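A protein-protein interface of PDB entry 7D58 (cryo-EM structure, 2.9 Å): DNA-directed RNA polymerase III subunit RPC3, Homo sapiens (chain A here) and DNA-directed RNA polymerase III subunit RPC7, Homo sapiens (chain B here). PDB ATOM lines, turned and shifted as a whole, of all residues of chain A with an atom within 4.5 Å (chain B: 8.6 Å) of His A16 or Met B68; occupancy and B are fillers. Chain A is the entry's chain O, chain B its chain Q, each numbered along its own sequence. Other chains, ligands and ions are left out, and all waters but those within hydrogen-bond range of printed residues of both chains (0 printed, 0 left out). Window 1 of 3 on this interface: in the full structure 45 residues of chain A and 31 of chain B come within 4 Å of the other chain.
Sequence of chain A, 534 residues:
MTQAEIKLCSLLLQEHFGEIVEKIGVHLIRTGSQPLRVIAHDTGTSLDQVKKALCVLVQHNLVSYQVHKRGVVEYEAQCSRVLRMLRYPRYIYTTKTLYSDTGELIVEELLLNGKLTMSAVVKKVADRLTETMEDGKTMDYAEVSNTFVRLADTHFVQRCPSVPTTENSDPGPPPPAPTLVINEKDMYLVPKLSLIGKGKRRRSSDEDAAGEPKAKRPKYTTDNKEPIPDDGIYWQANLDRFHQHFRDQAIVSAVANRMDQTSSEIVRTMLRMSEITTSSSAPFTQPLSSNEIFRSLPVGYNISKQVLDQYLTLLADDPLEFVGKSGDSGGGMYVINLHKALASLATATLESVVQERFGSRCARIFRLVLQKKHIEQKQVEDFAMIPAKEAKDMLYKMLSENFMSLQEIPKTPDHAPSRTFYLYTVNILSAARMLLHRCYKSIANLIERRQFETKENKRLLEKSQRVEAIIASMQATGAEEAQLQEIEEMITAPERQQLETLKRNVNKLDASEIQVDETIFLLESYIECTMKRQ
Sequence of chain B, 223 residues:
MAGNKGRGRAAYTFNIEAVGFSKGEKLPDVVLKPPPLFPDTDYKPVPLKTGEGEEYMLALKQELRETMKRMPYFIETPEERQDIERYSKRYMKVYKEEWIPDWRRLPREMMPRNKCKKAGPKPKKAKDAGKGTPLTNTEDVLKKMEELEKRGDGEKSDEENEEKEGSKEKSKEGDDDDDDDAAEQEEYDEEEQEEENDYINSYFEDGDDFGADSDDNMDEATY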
ATOM      1  N   LEU A  12      22.861  -9.556  27.310  1.00  0.00           N
ATOM      2  CA  LEU A  12      22.262 -10.779  26.789  1.00  0.00           C
ATOM      3  C   LEU A  12      20.883 -10.524  26.193  1.00  0.00           C
ATOM      4  O   LEU A  12      20.482 -11.215  25.251  1.00  0.00           O
ATOM      5  CB  LEU A  12      22.176 -11.834  27.892  1.00  0.00           C
ATOM      6  CG  LEU A  12      23.487 -12.537  28.250  1.00  0.00           C
ATOM      7  CD1 LEU A  12      23.263 -13.598  29.318  1.00  0.00           C
ATOM      8  CD2 LEU A  12      24.120 -13.142  27.009  1.00  0.00           C
ATOM      9  N   LEU A  13      20.150  -9.544  26.720  1.00  0.00           N
ATOM     10  CA  LEU A  13      18.851  -9.168  26.182  1.00  0.00           C
ATOM     11  C   LEU A  13      18.934  -8.051  25.152  1.00  0.00           C
ATOM     12  O   LEU A  13      17.965  -7.835  24.417  1.00  0.00           O
ATOM     13  CB  LEU A  13      17.904  -8.744  27.315  1.00  0.00           C
ATOM     14  CG  LEU A  13      16.968  -9.828  27.854  1.00  0.00           C
ATOM     15  CD1 LEU A  13      17.754 -10.919  28.558  1.00  0.00           C
ATOM     16  CD2 LEU A  13      15.920  -9.231  28.785  1.00  0.00           C
ATOM     17  N   GLN A  14      20.057  -7.338  25.082  1.00  0.00           N
ATOM     18  CA  GLN A  14      20.277  -6.366  24.024  1.00  0.00           C
ATOM     19  C   GLN A  14      20.763  -7.005  22.730  1.00  0.00           C
ATOM     20  O   GLN A  14      20.461  -6.487  21.648  1.00  0.00           O
ATOM     21  CB  GLN A  14      21.286  -5.307  24.481  1.00  0.00           C
ATOM     22  CG  GLN A  14      21.395  -4.110  23.553  1.00  0.00           C
ATOM     23  CD  GLN A  14      22.501  -3.160  23.960  1.00  0.00           C
ATOM     24  OE1 GLN A  14      23.238  -2.649  23.116  1.00  0.00           O
ATOM     25  NE2 GLN A  14      22.624  -2.916  25.259  1.00  0.00           N
ATOM     26  N   GLU A  15      21.500  -8.113  22.811  1.00  0.00           N
ATOM     27  CA  GLU A  15      21.928  -8.840  21.622  1.00  0.00           C
ATOM     28  C   GLU A  15      20.952  -9.921  21.184  1.00  0.00           C
ATOM     29  O   GLU A  15      20.947 -10.287  20.008  1.00  0.00           O
ATOM     30  CB  GLU A  15      23.309  -9.472  21.849  1.00  0.00           C
ATOM     31  CG  GLU A  15      23.310 -10.649  22.806  1.00  0.00           C
ATOM     32  CD  GLU A  15      24.550 -11.510  22.673  1.00  0.00           C
ATOM     33  OE1 GLU A  15      24.666 -12.504  23.419  1.00  0.00           O
ATOM     34  OE2 GLU A  15      25.408 -11.192  21.823  1.00  0.00           O
ATOM     35  N   HIS A  16      20.129 -10.440  22.097  1.00  0.00           N
ATOM     36  CA  HIS A  16      19.096 -11.406  21.743  1.00  0.00           C
ATOM     37  C   HIS A  16      17.785 -10.717  21.379  1.00  0.00           C
ATOM     38  O   HIS A  16      17.225 -10.965  20.307  1.00  0.00           O
ATOM     39  CB  HIS A  16      18.869 -12.389  22.896  1.00  0.00           C
ATOM     40  CG  HIS A  16      19.926 -13.444  23.014  1.00  0.00           C
ATOM     41  ND1 HIS A  16      19.628 -14.786  23.113  1.00  0.00           N
ATOM     42  CD2 HIS A  16      21.276 -13.355  23.045  1.00  0.00           C
ATOM     43  CE1 HIS A  16      20.749 -15.479  23.204  1.00  0.00           C
ATOM     44  NE2 HIS A  16      21.764 -14.634  23.164  1.00  0.00           N
ATOM     45  N   PHE A  17      17.285  -9.856  22.265  1.00  0.00           N
ATOM     46  CA  PHE A  17      16.078  -9.077  22.061  1.00  0.00           C
ATOM     47  C   PHE A  17      16.471  -7.641  21.699  1.00  0.00           C
ATOM     48  O   PHE A  17      17.671  -7.348  21.541  1.00  0.00           O
ATOM     49  CB  PHE A  17      15.204  -9.185  23.307  1.00  0.00           C
ATOM     50  CG  PHE A  17      14.703 -10.575  23.581  1.00  0.00           C
ATOM     51  CD1 PHE A  17      15.364 -11.398  24.479  1.00  0.00           C
ATOM     52  CD2 PHE A  17      13.572 -11.057  22.944  1.00  0.00           C
ATOM     53  CE1 PHE A  17      14.905 -12.677  24.735  1.00  0.00           C
ATOM     54  CE2 PHE A  17      13.110 -12.336  23.196  1.00  0.00           C
ATOM     55  CZ  PHE A  17      13.777 -13.146  24.093  1.00  0.00           C
ATOM     56  N   MET A  85      20.556 -18.591  29.009  1.00  0.00           N
ATOM     57  CA  MET A  85      20.532 -18.480  27.557  1.00  0.00           C
ATOM     58  C   MET A  85      21.882 -18.776  26.921  1.00  0.00           C
ATOM     59  O   MET A  85      21.966 -18.867  25.692  1.00  0.00           O
ATOM     60  CB  MET A  85      20.059 -17.083  27.141  1.00  0.00           C
ATOM     61  CG  MET A  85      18.563 -16.864  27.299  1.00  0.00           C
ATOM     62  SD  MET A  85      18.020 -15.273  26.648  1.00  0.00           S
ATOM     63  CE  MET A  85      16.241 -15.453  26.758  1.00  0.00           C
ATOM     64  N   LEU A 112      13.203 -20.862  21.120  1.00  0.00           N
ATOM     65  CA  LEU A 112      13.140 -19.587  20.421  1.00  0.00           C
ATOM     66  C   LEU A 112      11.746 -18.977  20.433  1.00  0.00           C
ATOM     67  O   LEU A 112      11.608 -17.780  20.158  1.00  0.00           O
ATOM     68  CB  LEU A 112      13.608 -19.753  18.969  1.00  0.00           C
ATOM     69  CG  LEU A 112      15.118 -19.877  18.747  1.00  0.00           C
ATOM     70  CD1 LEU A 112      15.441 -19.882  17.261  1.00  0.00           C
ATOM     71  CD2 LEU A 112      15.860 -18.755  19.456  1.00  0.00           C
ATOM     72  N   LYS B  61      25.309 -21.591  17.816  1.00  0.00           N
ATOM     73  CA  LYS B  61      25.106 -20.316  18.495  1.00  0.00           C
ATOM     74  C   LYS B  61      25.140 -19.153  17.512  1.00  0.00           C
ATOM     75  O   LYS B  61      24.336 -18.216  17.627  1.00  0.00           O
ATOM     76  CB  LYS B  61      26.167 -20.137  19.583  1.00  0.00           C
ATOM     77  CG  LYS B  61      26.344 -18.712  20.081  1.00  0.00           C
ATOM     78  CD  LYS B  61      26.762 -18.700  21.545  1.00  0.00           C
ATOM     79  CE  LYS B  61      28.272 -18.816  21.691  1.00  0.00           C
ATOM     80  NZ  LYS B  61      28.709 -18.619  23.102  1.00  0.00           N
ATOM     81  N   GLN B  62      26.049 -19.205  16.533  1.00  0.00           N
ATOM     82  CA  GLN B  62      26.150 -18.131  15.549  1.00  0.00           C
ATOM     83  C   GLN B  62      24.908 -18.051  14.670  1.00  0.00           C
ATOM     84  O   GLN B  62      24.572 -16.968  14.175  1.00  0.00           O
ATOM     85  CB  GLN B  62      27.398 -18.324  14.687  1.00  0.00           C
ATOM     86  CG  GLN B  62      28.673 -17.753  15.290  1.00  0.00           C
ATOM     87  CD  GLN B  62      29.920 -18.208  14.554  1.00  0.00           C
ATOM     88  OE1 GLN B  62      31.035 -17.811  14.891  1.00  0.00           O
ATOM     89  NE2 GLN B  62      29.735 -19.045  13.540  1.00  0.00           N
ATOM     90  N   GLU B  63      24.219 -19.174  14.457  1.00  0.00           N
ATOM     91  CA  GLU B  63      22.967 -19.139  13.711  1.00  0.00           C
ATOM     92  C   GLU B  63      21.766 -18.825  14.595  1.00  0.00           C
ATOM     93  O   GLU B  63      20.820 -18.185  14.125  1.00  0.00           O
ATOM     94  CB  GLU B  63      22.749 -20.460  12.960  1.00  0.00           C
ATOM     95  CG  GLU B  63      22.455 -21.678  13.825  1.00  0.00           C
ATOM     96  CD  GLU B  63      20.975 -21.870  14.098  1.00  0.00           C
ATOM     97  OE1 GLU B  63      20.150 -21.346  13.320  1.00  0.00           O
ATOM     98  OE2 GLU B  63      20.636 -22.548  15.092  1.00  0.00           O
ATOM     99  N   LEU B  64      21.781 -19.242  15.866  1.00  0.00           N
ATOM    100  CA  LEU B  64      20.709 -18.855  16.780  1.00  0.00           C
ATOM    101  C   LEU B  64      20.665 -17.347  16.966  1.00  0.00           C
ATOM    102  O   LEU B  64      19.587 -16.742  16.929  1.00  0.00           O
ATOM    103  CB  LEU B  64      20.877 -19.548  18.134  1.00  0.00           C
ATOM    104  CG  LEU B  64      20.576 -21.041  18.256  1.00  0.00           C
ATOM    105  CD1 LEU B  64      20.982 -21.537  19.634  1.00  0.00           C
ATOM    106  CD2 LEU B  64      19.101 -21.307  18.009  1.00  0.00           C
ATOM    107  N   ARG B  65      21.828 -16.720  17.175  1.00  0.00           N
ATOM    108  CA  ARG B  65      21.858 -15.268  17.317  1.00  0.00           C
ATOM    109  C   ARG B  65      21.339 -14.572  16.064  1.00  0.00           C
ATOM    110  O   ARG B  65      20.527 -13.645  16.163  1.00  0.00           O
ATOM    111  CB  ARG B  65      23.279 -14.801  17.640  1.00  0.00           C
ATOM    112  CG  ARG B  65      23.598 -13.387  17.182  1.00  0.00           C
ATOM    113  CD  ARG B  65      25.045 -13.032  17.477  1.00  0.00           C
ATOM    114  NE  ARG B  65      25.951 -13.507  16.435  1.00  0.00           N
ATOM    115  CZ  ARG B  65      27.204 -13.891  16.655  1.00  0.00           C
ATOM    116  NH1 ARG B  65      27.959 -14.308  15.648  1.00  0.00           N
ATOM    117  NH2 ARG B  65      27.702 -13.860  17.883  1.00  0.00           N
ATOM    118  N   GLU B  66      21.768 -15.024  14.883  1.00  0.00           N
ATOM    119  CA  GLU B  66      21.347 -14.371  13.648  1.00  0.00           C
ATOM    120  C   GLU B  66      19.861 -14.578  13.382  1.00  0.00           C
ATOM    121  O   GLU B  66      19.180 -13.669  12.893  1.00  0.00           O
ATOM    122  CB  GLU B  66      22.178 -14.884  12.471  1.00  0.00           C
ATOM    123  CG  GLU B  66      21.863 -14.196  11.153  1.00  0.00           C
ATOM    124  CD  GLU B  66      22.217 -12.721  11.168  1.00  0.00           C
ATOM    125  OE1 GLU B  66      23.141 -12.339  11.917  1.00  0.00           O
ATOM    126  OE2 GLU B  66      21.571 -11.944  10.434  1.00  0.00           O
ATOM    127  N   THR B  67      19.335 -15.763  13.700  1.00  0.00           N
ATOM    128  CA  THR B  67      17.928 -16.035  13.446  1.00  0.00           C
ATOM    129  C   THR B  67      17.017 -15.331  14.440  1.00  0.00           C
ATOM    130  O   THR B  67      15.951 -14.842  14.050  1.00  0.00           O
ATOM    131  CB  THR B  67      17.672 -17.543  13.472  1.00  0.00           C
ATOM    132  OG1 THR B  67      18.429 -18.138  14.532  1.00  0.00           O
ATOM    133  CG2 THR B  67      18.081 -18.176  12.146  1.00  0.00           C
ATOM    134  N   MET B  68      17.410 -15.252  15.714  1.00  0.00           N
ATOM    135  CA  MET B  68      16.595 -14.525  16.680  1.00  0.00           C
ATOM    136  C   MET B  68      16.764 -13.021  16.511  1.00  0.00           C
ATOM    137  O   MET B  68      15.943 -12.240  17.005  1.00  0.00           O
ATOM    138  CB  MET B  68      16.944 -14.955  18.105  1.00  0.00           C
ATOM    139  CG  MET B  68      18.153 -14.262  18.695  1.00  0.00           C
ATOM    140  SD  MET B  68      18.597 -14.977  20.285  1.00  0.00           S
ATOM    141  CE  MET B  68      17.005 -14.953  21.107  1.00  0.00           C
ATOM    142  N   LYS B  69      17.828 -12.596  15.824  1.00  0.00           N
ATOM    143  CA  LYS B  69      17.916 -11.202  15.405  1.00  0.00           C
ATOM    144  C   LYS B  69      16.926 -10.910  14.285  1.00  0.00           C
ATOM    145  O   LYS B  69      16.470  -9.770  14.131  1.00  0.00           O
ATOM    146  CB  LYS B  69      19.344 -10.877  14.963  1.00  0.00           C
ATOM    147  CG  LYS B  69      19.590  -9.401  14.688  1.00  0.00           C
ATOM    148  CD  LYS B  69      20.981  -9.168  14.121  1.00  0.00           C
ATOM    149  CE  LYS B  69      21.446  -7.743  14.372  1.00  0.00           C
ATOM    150  NZ  LYS B  69      22.877  -7.556  14.010  1.00  0.00           N
ATOM    151  N   ARG B  70      16.574 -11.928  13.502  1.00  0.00           N
ATOM    152  CA  ARG B  70      15.636 -11.803  12.387  1.00  0.00           C
ATOM    153  C   ARG B  70      14.261 -12.359  12.735  1.00  0.00           C
ATOM    154  O   ARG B  70      13.524 -12.808  11.852  1.00  0.00           O
ATOM    155  CB  ARG B  70      16.194 -12.496  11.149  1.00  0.00           C
ATOM    156  CG  ARG B  70      17.511 -11.926  10.645  1.00  0.00           C
ATOM    157  CD  ARG B  70      17.293 -10.699   9.774  1.00  0.00           C
ATOM    158  NE  ARG B  70      17.151  -9.479  10.565  1.00  0.00           N
ATOM    159  CZ  ARG B  70      18.172  -8.783  11.054  1.00  0.00           C
ATOM    160  NH1 ARG B  70      17.948  -7.686  11.763  1.00  0.00           N
ATOM    161  NH2 ARG B  70      19.418  -9.182  10.834  1.00  0.00           N
ATOM    162  N   MET B  71      13.892 -12.344  14.006  1.00  0.00           N
ATOM    163  CA  MET B  71      12.601 -12.810  14.479  1.00  0.00           C
ATOM    164  C   MET B  71      11.678 -11.635  14.769  1.00  0.00           C
ATOM    165  O   MET B  71      12.134 -10.523  15.058  1.00  0.00           O
ATOM    166  CB  MET B  71      12.771 -13.664  15.742  1.00  0.00           C
ATOM    167  CG  MET B  71      13.165 -15.109  15.471  1.00  0.00           C
ATOM    168  SD  MET B  71      11.930 -16.024  14.529  1.00  0.00           S
ATOM    169  CE  MET B  71      10.647 -16.242  15.759  1.00  0.00           C
ATOM    170  N   PRO B  72      10.358 -11.842  14.690  1.00  0.00           N
ATOM    171  CA  PRO B  72       9.422 -10.756  15.012  1.00  0.00           C
ATOM    172  C   PRO B  72       9.493 -10.345  16.474  1.00  0.00           C
ATOM    173  O   PRO B  72       9.187  -9.198  16.816  1.00  0.00           O
ATOM    174  CB  PRO B  72       8.053 -11.352  14.658  1.00  0.00           C
ATOM    175  CG  PRO B  72       8.258 -12.832  14.691  1.00  0.00           C
ATOM    176  CD  PRO B  72       9.661 -13.051  14.220  1.00  0.00           C
ATOM    177  N   TYR B  73       9.892 -11.276  17.344  1.00  0.00           N
ATOM    178  CA  TYR B  73      10.043 -10.954  18.759  1.00  0.00           C
ATOM    179  C   TYR B  73      11.132  -9.908  18.966  1.00  0.00           C
ATOM    180  O   TYR B  73      11.018  -9.042  19.842  1.00  0.00           O
ATOM    181  CB  TYR B  73      10.347 -12.221  19.557  1.00  0.00           C
ATOM    182  CG  TYR B  73       9.280 -13.286  19.442  1.00  0.00           C
ATOM    183  CD1 TYR B  73       8.070 -13.160  20.112  1.00  0.00           C
ATOM    184  CD2 TYR B  73       9.482 -14.418  18.664  1.00  0.00           C
ATOM    185  CE1 TYR B  73       7.091 -14.130  20.009  1.00  0.00           C
ATOM    186  CE2 TYR B  73       8.509 -15.394  18.555  1.00  0.00           C
ATOM    187  CZ  TYR B  73       7.317 -15.245  19.229  1.00  0.00           C
ATOM    188  OH  TYR B  73       6.345 -16.215  19.124  1.00  0.00           O
ATOM    189  N   PHE B  74      12.197  -9.976  18.169  1.00  0.00           N
ATOM    190  CA  PHE B  74      13.242  -8.961  18.200  1.00  0.00           C
ATOM    191  C   PHE B  74      12.707  -7.651  17.641  1.00  0.00           C
ATOM    192  O   PHE B  74      12.375  -7.565  16.455  1.00  0.00           O
ATOM    193  CB  PHE B  74      14.468  -9.424  17.408  1.00  0.00           C
ATOM    194  CG  PHE B  74      15.604  -8.439  17.411  1.00  0.00           C
ATOM    195  CD1 PHE B  74      16.545  -8.451  18.426  1.00  0.00           C
ATOM    196  CD2 PHE B  74      15.736  -7.509  16.393  1.00  0.00           C
ATOM    197  CE1 PHE B  74      17.593  -7.548  18.429  1.00  0.00           C
ATOM    198  CE2 PHE B  74      16.780  -6.604  16.391  1.00  0.00           C
ATOM    199  CZ  PHE B  74      17.710  -6.624  17.412  1.00  0.00           C
ATOM    200  N   ILE B  75      12.607  -6.629  18.488  1.00  0.00           N
ATOM    201  CA  ILE B  75      12.093  -5.335  18.057  1.00  0.00           C
ATOM    202  C   ILE B  75      13.224  -4.517  17.450  1.00  0.00           C
ATOM    203  O   ILE B  75      14.023  -3.908  18.172  1.00  0.00           O
ATOM    204  CB  ILE B  75      11.429  -4.585  19.226  1.00  0.00           C
ATOM    205  CG1 ILE B  75      10.260  -5.401  19.780  1.00  0.00           C
ATOM    206  CG2 ILE B  75      10.952  -3.211  18.777  1.00  0.00           C
ATOM    207  CD1 ILE B  75       9.694  -4.856  21.070  1.00  0.00           C
ATOM    208  N   GLU B  76      13.302  -4.498  16.122  1.00  0.00           N
ATOM    209  CA  GLU B  76      14.269  -3.678  15.407  1.00  0.00           C
ATOM    210  C   GLU B  76      13.671  -2.354  14.957  1.00  0.00           C
ATOM    211  O   GLU B  76      14.258  -1.673  14.110  1.00  0.00           O
ATOM    212  CB  GLU B  76      14.827  -4.439  14.201  1.00  0.00           C
ATOM    213  CG  GLU B  76      13.808  -4.718  13.106  1.00  0.00           C
ATOM    214  CD  GLU B  76      13.295  -6.145  13.132  1.00  0.00           C
ATOM    215  OE1 GLU B  76      13.630  -6.882  14.081  1.00  0.00           O
ATOM    216  OE2 GLU B  76      12.557  -6.531  12.201  1.00  0.00           O
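Of the 16 printed residues of chain B, 3 touch a printed residue of chain A. Along chain B the printed residues that touch a printed residue of chain A span positions 64 to 74. Of the 8 printed residues of chain A, 3 touch a printed residue of chain B. Hydrophobic or aromatic side chains of chain A that line the printed part of chain B: His A16 and Leu A112. Among the printed residues, 4 pairs touch across the chains. Among the printed residues, no Asp or Glu carboxylate lies within 4 Å of a Lys or Arg side-chain nitrogen of the other chain.
The side-chain hydroxyl of Thr B67 is in hydrogen-bond range of the backbone carbonyl oxygen of Leu B64 (3.0 Å).
A ring nitrogen (ND1) of His A16 sits at hydrogen-bond distance from the side-chain sulfur of Met B68, at 3.0 Å.
Of chain B, only Met B68 (3.0 Å) and Phe B74 (3.2 Å) come within 4 Å of His A16. Printed residues of chain B within 4 Å of Phe A17: Phe B74 (3.1 Å). Printed residues of chain B within 4 Å of Leu A112: Leu B64 (3.998 Å). Printed residues of chain A within 4 Å of Leu B64: Leu A112 (3.998 Å). Of chain A, only His A16 (3.0 Å) comes within 4 Å of Met B68. Met B71 touches none of the printed residues of chain A. Of the printed residues of chain A, Phe B74 touches His A16 and Phe A17. Glu B76 touches none of the printed residues of chain A. The nearest residue of chain B that does not touch His A16 is Lys B69 (4.8 Å). The nearest residue of chain A that does not touch Met B68 is Leu A112 (4.2 Å).
Among the printed residues, pairs that only touch across the chains: Phe A17 with Phe B74 (3.1 Å), His A16 with Phe B74 (3.2 Å) and Leu A112 with Leu B64 (3.998 Å).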
